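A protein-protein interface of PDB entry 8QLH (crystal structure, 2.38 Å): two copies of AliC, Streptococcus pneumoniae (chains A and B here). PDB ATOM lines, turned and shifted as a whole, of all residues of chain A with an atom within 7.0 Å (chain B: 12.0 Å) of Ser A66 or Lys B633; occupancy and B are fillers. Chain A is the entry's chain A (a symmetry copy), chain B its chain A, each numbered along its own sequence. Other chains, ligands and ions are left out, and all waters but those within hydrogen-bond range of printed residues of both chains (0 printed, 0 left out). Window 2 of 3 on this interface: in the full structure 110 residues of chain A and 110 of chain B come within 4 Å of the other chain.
A ring nitrogen (ND1) of His B631 is in hydrogen-bond range of the backbone carbonyl oxygen (O) of Trp A63. The backbone NH (N) of Lys B633 lies within hydrogen-bond range of the backbone carbonyl oxygen (O) of Val A65 (3.0 Å). O of His B631 sits at hydrogen-bond distance from N of Val A65 (2.8 Å).
N of Ser A64 lies within hydrogen-bond range of O of Thr A73, 2.8 Å away. OD1 of Asp A68 sits at hydrogen-bond distance from OG of Ser A66 (2.7 Å). The backbone NH of Ser A66 sits at hydrogen-bond distance from the backbone carbonyl oxygen of Thr A71, at 2.9 Å. A ring nitrogen (NE2) of His B631 sits at hydrogen-bond distance from the side-chain amino group (NZ) of Lys B630.
Among the printed residues, pairs that only touch across the chains: Asp A62 with His B631 (3.8 Å), Trp A63 with Leu B628 (3.9 Å), Ser A64 with His B631 (3.2 Å), Ser A64 with Lys B633 (3.5 Å), Val A65 with Ile B632 (3.4 Å) and Ser A66 with Lys B633 (3.3 Å).
Ser A66 touches just one residue of chain B: Lys B633. Of the printed residues of chain A, Lys B633 touches Ser A64 (3.5 Å), Val A65 (3.0 Å) and Ser A66 (3.3 Å). Ser A64 touches just these residues of chain B: His B631 and Lys B633. No residue of chain B comes within 4 Å of Lys A67. No residue of chain B comes within 4 Å of Asp A68. Leu A70 touches none of the printed residues of chain B. Thr A71 touches none of the printed residues of chain B. No residue of chain B comes within 4 Å of Tyr A72. Of the printed residues of chain A, Ile B632 touches Val A65 (3.4 Å). Of the printed residues of chain B, Trp A63 touches Leu B628 and His B631. Of the printed residues of chain A, Leu B628 touches Trp A63. Thr B534 touches none of the printed residues of chain A. Asn B536 touches none of the printed residues of chain A. The nearest residue of chain A that does not touch Lys B633 is Lys A67 (4.3 Å). The nearest printed residue of chain B that does not touch Trp A63 is Lys B633 (5.9 Å).
Of the 13 printed residues of chain A, 5 touch a printed residue of chain B. Printed residues of chain A that touch a printed residue of chain B: Asp A62, Trp A63, Ser A64, Val A65 and Ser A66. Hydrophobic or aromatic side chains of chain A that line the printed part of chain B: Trp A63 and Val A65. Hydrophobic or aromatic side chains of chain B within 4 Å of the printed part of chain A: Leu B628, His B631 and Ile B632. Among the printed residues, 9 pairs touch across the chains.
No position is printed for both chains. Of the 9 pairs that touch across the chains among the printed residues, none has its exchanged pair printed and touching as well.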
ATOM      1  N   ASP A  62       1.948  38.793  -7.724  1.00  0.00           N
ATOM      2  CA  ASP A  62       0.713  38.089  -7.413  1.00  0.00           C
ATOM      3  C   ASP A  62       1.079  36.729  -6.838  1.00  0.00           C
ATOM      4  O   ASP A  62       2.198  36.242  -7.019  1.00  0.00           O
ATOM      5  CB  ASP A  62      -0.186  37.945  -8.648  1.00  0.00           C
ATOM      6  CG  ASP A  62      -1.649  37.751  -8.283  1.00  0.00           C
ATOM      7  OD1 ASP A  62      -1.962  37.712  -7.072  1.00  0.00           O
ATOM      8  OD2 ASP A  62      -2.484  37.626  -9.206  1.00  0.00           O
ATOM      9  N   TRP A  63       0.124  36.125  -6.131  1.00  0.00           N
ATOM     10  CA  TRP A  63       0.352  34.827  -5.515  1.00  0.00           C
ATOM     11  C   TRP A  63      -0.963  34.071  -5.419  1.00  0.00           C
ATOM     12  O   TRP A  63      -2.043  34.665  -5.348  1.00  0.00           O
ATOM     13  CB  TRP A  63       0.984  34.957  -4.121  1.00  0.00           C
ATOM     14  CG  TRP A  63       0.107  35.619  -3.107  1.00  0.00           C
ATOM     15  CD1 TRP A  63       0.056  36.954  -2.815  1.00  0.00           C
ATOM     16  CD2 TRP A  63      -0.842  34.984  -2.242  1.00  0.00           C
ATOM     17  NE1 TRP A  63      -0.868  37.187  -1.829  1.00  0.00           N
ATOM     18  CE2 TRP A  63      -1.432  35.996  -1.456  1.00  0.00           C
ATOM     19  CE3 TRP A  63      -1.250  33.661  -2.054  1.00  0.00           C
ATOM     20  CZ2 TRP A  63      -2.410  35.726  -0.499  1.00  0.00           C
ATOM     21  CZ3 TRP A  63      -2.220  33.394  -1.103  1.00  0.00           C
ATOM     22  CH2 TRP A  63      -2.791  34.422  -0.340  1.00  0.00           C
ATOM     23  N   SER A  64      -0.856  32.745  -5.390  1.00  0.00           N
ATOM     24  CA  SER A  64      -2.024  31.889  -5.283  1.00  0.00           C
ATOM     25  C   SER A  64      -1.709  30.724  -4.356  1.00  0.00           C
ATOM     26  O   SER A  64      -0.547  30.393  -4.115  1.00  0.00           O
ATOM     27  CB  SER A  64      -2.474  31.375  -6.656  1.00  0.00           C
ATOM     28  OG  SER A  64      -1.844  30.147  -6.973  1.00  0.00           O
ATOM     29  N   VAL A  65      -2.768  30.108  -3.829  1.00  0.00           N
ATOM     30  CA  VAL A  65      -2.670  28.902  -3.014  1.00  0.00           C
ATOM     31  C   VAL A  65      -3.646  27.870  -3.573  1.00  0.00           C
ATOM     32  O   VAL A  65      -4.732  28.226  -4.047  1.00  0.00           O
ATOM     33  CB  VAL A  65      -2.943  29.202  -1.519  1.00  0.00           C
ATOM     34  CG1 VAL A  65      -4.321  29.835  -1.318  1.00  0.00           C
ATOM     35  CG2 VAL A  65      -2.769  27.957  -0.650  1.00  0.00           C
ATOM     36  N   SER A  66      -3.248  26.594  -3.554  1.00  0.00           N
ATOM     37  CA  SER A  66      -4.092  25.543  -4.107  1.00  0.00           C
ATOM     38  C   SER A  66      -5.342  25.355  -3.243  1.00  0.00           C
ATOM     39  O   SER A  66      -5.443  25.868  -2.126  1.00  0.00           O
ATOM     40  CB  SER A  66      -3.331  24.218  -4.213  1.00  0.00           C
ATOM     41  OG  SER A  66      -2.527  23.984  -3.075  1.00  0.00           O
ATOM     42  N   LYS A  67      -6.297  24.585  -3.775  1.00  0.00           N
ATOM     43  CA  LYS A  67      -7.543  24.327  -3.055  1.00  0.00           C
ATOM     44  C   LYS A  67      -7.292  23.598  -1.738  1.00  0.00           C
ATOM     45  O   LYS A  67      -7.981  23.848  -0.742  1.00  0.00           O
ATOM     46  CB  LYS A  67      -8.505  23.519  -3.934  1.00  0.00           C
ATOM     47  CG  LYS A  67      -9.316  24.338  -4.940  1.00  0.00           C
ATOM     48  CD  LYS A  67      -9.547  23.556  -6.230  1.00  0.00           C
ATOM     49  CE  LYS A  67     -10.871  23.915  -6.891  1.00  0.00           C
ATOM     50  NZ  LYS A  67     -10.951  25.365  -7.213  1.00  0.00           N
ATOM     51  N   ASP A  68      -6.320  22.685  -1.710  1.00  0.00           N
ATOM     52  CA  ASP A  68      -6.007  21.960  -0.486  1.00  0.00           C
ATOM     53  C   ASP A  68      -5.108  22.742   0.464  1.00  0.00           C
ATOM     54  O   ASP A  68      -4.834  22.260   1.567  1.00  0.00           O
ATOM     55  CB  ASP A  68      -5.372  20.600  -0.816  1.00  0.00           C
ATOM     56  CG  ASP A  68      -4.048  20.716  -1.558  1.00  0.00           C
ATOM     57  OD1 ASP A  68      -3.636  21.840  -1.917  1.00  0.00           O
ATOM     58  OD2 ASP A  68      -3.416  19.664  -1.791  1.00  0.00           O
ATOM     59  N   GLY A  69      -4.637  23.923   0.068  1.00  0.00           N
ATOM     60  CA  GLY A  69      -3.831  24.763   0.934  1.00  0.00           C
ATOM     61  C   GLY A  69      -2.375  24.378   1.065  1.00  0.00           C
ATOM     62  O   GLY A  69      -1.655  25.010   1.847  1.00  0.00           O
ATOM     63  N   LEU A  70      -1.905  23.379   0.322  1.00  0.00           N
ATOM     64  CA  LEU A  70      -0.550  22.875   0.511  1.00  0.00           C
ATOM     65  C   LEU A  70       0.473  23.507  -0.420  1.00  0.00           C
ATOM     66  O   LEU A  70       1.676  23.382  -0.163  1.00  0.00           O
ATOM     67  CB  LEU A  70      -0.518  21.358   0.310  1.00  0.00           C
ATOM     68  CG  LEU A  70      -1.402  20.543   1.250  1.00  0.00           C
ATOM     69  CD1 LEU A  70      -1.463  19.082   0.829  1.00  0.00           C
ATOM     70  CD2 LEU A  70      -0.879  20.676   2.668  1.00  0.00           C
ATOM     71  N   THR A  71       0.039  24.170  -1.490  1.00  0.00           N
ATOM     72  CA  THR A  71       0.942  24.675  -2.518  1.00  0.00           C
ATOM     73  C   THR A  71       0.727  26.169  -2.691  1.00  0.00           C
ATOM     74  O   THR A  71      -0.384  26.607  -3.011  1.00  0.00           O
ATOM     75  CB  THR A  71       0.731  23.957  -3.853  1.00  0.00           C
ATOM     76  OG1 THR A  71       1.057  22.571  -3.709  1.00  0.00           O
ATOM     77  CG2 THR A  71       1.612  24.573  -4.925  1.00  0.00           C
ATOM     78  N   TYR A  72       1.793  26.939  -2.498  1.00  0.00           N
ATOM     79  CA  TYR A  72       1.776  28.385  -2.661  1.00  0.00           C
ATOM     80  C   TYR A  72       2.660  28.753  -3.841  1.00  0.00           C
ATOM     81  O   TYR A  72       3.818  28.330  -3.906  1.00  0.00           O
ATOM     82  CB  TYR A  72       2.271  29.090  -1.400  1.00  0.00           C
ATOM     83  CG  TYR A  72       1.276  29.128  -0.265  1.00  0.00           C
ATOM     84  CD1 TYR A  72       1.113  28.042   0.583  1.00  0.00           C
ATOM     85  CD2 TYR A  72       0.507  30.263  -0.032  1.00  0.00           C
ATOM     86  CE1 TYR A  72       0.206  28.086   1.637  1.00  0.00           C
ATOM     87  CE2 TYR A  72      -0.400  30.316   1.008  1.00  0.00           C
ATOM     88  CZ  TYR A  72      -0.548  29.226   1.840  1.00  0.00           C
ATOM     89  OH  TYR A  72      -1.455  29.281   2.872  1.00  0.00           O
ATOM     90  N   THR A  73       2.119  29.543  -4.762  1.00  0.00           N
ATOM     91  CA  THR A  73       2.817  29.904  -5.986  1.00  0.00           C
ATOM     92  C   THR A  73       2.887  31.420  -6.085  1.00  0.00           C
ATOM     93  O   THR A  73       1.870  32.104  -5.919  1.00  0.00           O
ATOM     94  CB  THR A  73       2.111  29.307  -7.206  1.00  0.00           C
ATOM     95  OG1 THR A  73       1.971  27.893  -7.027  1.00  0.00           O
ATOM     96  CG2 THR A  73       2.916  29.563  -8.455  1.00  0.00           C
ATOM     97  N   TYR A 149       6.073  26.939  -3.358  1.00  0.00           N
ATOM     98  CA  TYR A 149       6.342  26.293  -2.084  1.00  0.00           C
ATOM     99  C   TYR A 149       5.292  25.222  -1.828  1.00  0.00           C
ATOM    100  O   TYR A 149       4.096  25.442  -2.051  1.00  0.00           O
ATOM    101  CB  TYR A 149       6.340  27.305  -0.934  1.00  0.00           C
ATOM    102  CG  TYR A 149       7.505  28.268  -0.930  1.00  0.00           C
ATOM    103  CD1 TYR A 149       8.729  27.908  -0.381  1.00  0.00           C
ATOM    104  CD2 TYR A 149       7.374  29.546  -1.454  1.00  0.00           C
ATOM    105  CE1 TYR A 149       9.795  28.795  -0.365  1.00  0.00           C
ATOM    106  CE2 TYR A 149       8.428  30.437  -1.438  1.00  0.00           C
ATOM    107  CZ  TYR A 149       9.636  30.057  -0.895  1.00  0.00           C
ATOM    108  OH  TYR A 149      10.685  30.946  -0.890  1.00  0.00           O
ATOM    109  N   THR B 534      -7.334  23.758   9.986  1.00  0.00           N
ATOM    110  CA  THR B 534      -6.264  24.181   9.093  1.00  0.00           C
ATOM    111  C   THR B 534      -6.701  25.191   8.032  1.00  0.00           C
ATOM    112  O   THR B 534      -5.844  25.880   7.461  1.00  0.00           O
ATOM    113  CB  THR B 534      -5.658  22.958   8.400  1.00  0.00           C
ATOM    114  OG1 THR B 534      -6.701  22.103   7.895  1.00  0.00           O
ATOM    115  CG2 THR B 534      -4.784  22.160   9.358  1.00  0.00           C
ATOM    116  N   SER B 535      -7.996  25.308   7.769  1.00  0.00           N
ATOM    117  CA  SER B 535      -8.496  26.127   6.672  1.00  0.00           C
ATOM    118  C   SER B 535      -9.557  27.117   7.122  1.00  0.00           C
ATOM    119  O   SER B 535      -9.495  28.289   6.739  1.00  0.00           O
ATOM    120  CB  SER B 535      -9.055  25.227   5.552  1.00  0.00           C
ATOM    121  OG  SER B 535      -9.664  24.067   6.094  1.00  0.00           O
ATOM    122  N   ASN B 536     -10.544  26.677   7.904  1.00  0.00           N
ATOM    123  CA  ASN B 536     -11.641  27.539   8.351  1.00  0.00           C
ATOM    124  C   ASN B 536     -11.112  28.511   9.400  1.00  0.00           C
ATOM    125  O   ASN B 536     -10.897  28.138  10.554  1.00  0.00           O
ATOM    126  CB  ASN B 536     -12.784  26.694   8.908  1.00  0.00           C
ATOM    127  CG  ASN B 536     -14.095  27.452   8.991  1.00  0.00           C
ATOM    128  OD1 ASN B 536     -14.136  28.596   9.440  1.00  0.00           O
ATOM    129  ND2 ASN B 536     -15.177  26.810   8.556  1.00  0.00           N
ATOM    130  N   ASP B 627     -10.916  39.164   0.650  1.00  0.00           N
ATOM    131  CA  ASP B 627     -10.218  39.025  -0.614  1.00  0.00           C
ATOM    132  C   ASP B 627      -9.243  37.859  -0.625  1.00  0.00           C
ATOM    133  O   ASP B 627      -8.607  37.627  -1.651  1.00  0.00           O
ATOM    134  CB  ASP B 627      -9.473  40.325  -0.947  1.00  0.00           C
ATOM    135  CG  ASP B 627     -10.414  41.472  -1.261  1.00  0.00           C
ATOM    136  OD1 ASP B 627     -11.605  41.214  -1.537  1.00  0.00           O
ATOM    137  OD2 ASP B 627      -9.959  42.636  -1.224  1.00  0.00           O
ATOM    138  N   LEU B 628      -9.067  37.126   0.476  1.00  0.00           N
ATOM    139  CA  LEU B 628      -8.182  35.970   0.387  1.00  0.00           C
ATOM    140  C   LEU B 628      -8.785  34.881  -0.485  1.00  0.00           C
ATOM    141  O   LEU B 628      -8.046  34.042  -1.011  1.00  0.00           O
ATOM    142  CB  LEU B 628      -7.852  35.430   1.778  1.00  0.00           C
ATOM    143  CG  LEU B 628      -6.831  36.268   2.554  1.00  0.00           C
ATOM    144  CD1 LEU B 628      -6.631  35.694   3.939  1.00  0.00           C
ATOM    145  CD2 LEU B 628      -5.505  36.344   1.805  1.00  0.00           C
ATOM    146  N   GLU B 629     -10.105  34.915  -0.686  1.00  0.00           N
ATOM    147  CA  GLU B 629     -10.767  33.917  -1.516  1.00  0.00           C
ATOM    148  C   GLU B 629     -10.291  33.981  -2.963  1.00  0.00           C
ATOM    149  O   GLU B 629     -10.201  32.944  -3.627  1.00  0.00           O
ATOM    150  CB  GLU B 629     -12.291  34.098  -1.411  1.00  0.00           C
ATOM    151  CG  GLU B 629     -13.158  33.430  -2.499  1.00  0.00           C
ATOM    152  CD  GLU B 629     -13.189  34.195  -3.822  1.00  0.00           C
ATOM    153  OE1 GLU B 629     -13.715  33.646  -4.816  1.00  0.00           O
ATOM    154  OE2 GLU B 629     -12.655  35.327  -3.874  1.00  0.00           O
ATOM    155  N   LYS B 630      -9.995  35.179  -3.479  1.00  0.00           N
ATOM    156  CA  LYS B 630      -9.622  35.281  -4.886  1.00  0.00           C
ATOM    157  C   LYS B 630      -8.249  34.692  -5.175  1.00  0.00           C
ATOM    158  O   LYS B 630      -7.908  34.520  -6.350  1.00  0.00           O
ATOM    159  CB  LYS B 630      -9.677  36.743  -5.366  1.00  0.00           C
ATOM    160  CG  LYS B 630      -8.817  37.715  -4.588  1.00  0.00           C
ATOM    161  CD  LYS B 630      -8.793  39.140  -5.155  1.00  0.00           C
ATOM    162  CE  LYS B 630      -7.408  39.788  -5.061  1.00  0.00           C
ATOM    163  NZ  LYS B 630      -7.171  40.418  -3.720  1.00  0.00           N
ATOM    164  N   HIS B 631      -7.448  34.392  -4.152  1.00  0.00           N
ATOM    165  CA  HIS B 631      -6.134  33.797  -4.348  1.00  0.00           C
ATOM    166  C   HIS B 631      -6.155  32.275  -4.337  1.00  0.00           C
ATOM    167  O   HIS B 631      -5.085  31.659  -4.305  1.00  0.00           O
ATOM    168  CB  HIS B 631      -5.158  34.298  -3.283  1.00  0.00           C
ATOM    169  CG  HIS B 631      -4.952  35.779  -3.306  1.00  0.00           C
ATOM    170  ND1 HIS B 631      -3.959  36.379  -4.048  1.00  0.00           N
ATOM    171  CD2 HIS B 631      -5.608  36.780  -2.674  1.00  0.00           C
ATOM    172  CE1 HIS B 631      -4.015  37.688  -3.875  1.00  0.00           C
ATOM    173  NE2 HIS B 631      -5.008  37.957  -3.047  1.00  0.00           N
ATOM    174  N   ILE B 632      -7.334  31.656  -4.351  1.00  0.00           N
ATOM    175  CA  ILE B 632      -7.450  30.203  -4.424  1.00  0.00           C
ATOM    176  C   ILE B 632      -7.483  29.786  -5.886  1.00  0.00           C
ATOM    177  O   ILE B 632      -8.304  30.289  -6.664  1.00  0.00           O
ATOM    178  CB  ILE B 632      -8.710  29.702  -3.695  1.00  0.00           C
ATOM    179  CG1 ILE B 632      -8.886  30.402  -2.350  1.00  0.00           C
ATOM    180  CG2 ILE B 632      -8.666  28.177  -3.541  1.00  0.00           C
ATOM    181  CD1 ILE B 632      -8.174  29.730  -1.207  1.00  0.00           C
ATOM    182  N   LYS B 633      -6.596  28.868  -6.258  1.00  0.00           N
ATOM    183  CA  LYS B 633      -6.665  28.213  -7.559  1.00  0.00           C
ATOM    184  C   LYS B 633      -5.816  26.941  -7.556  1.00  0.00           C
ATOM    185  O   LYS B 633      -4.700  26.906  -7.038  1.00  0.00           O
ATOM    186  CB  LYS B 633      -6.232  29.169  -8.683  1.00  0.00           C
ATOM    187  CG  LYS B 633      -4.749  29.485  -8.767  1.00  0.00           C
ATOM    188  CD  LYS B 633      -4.364  29.822 -10.208  1.00  0.00           C
ATOM    189  CE  LYS B 633      -2.863  29.745 -10.430  1.00  0.00           C
ATOM    190  NZ  LYS B 633      -2.216  31.087 -10.374  1.00  0.00           N
ATOM    191  OXT LYS B 633      -6.242  25.898  -8.059  1.00  0.00           O
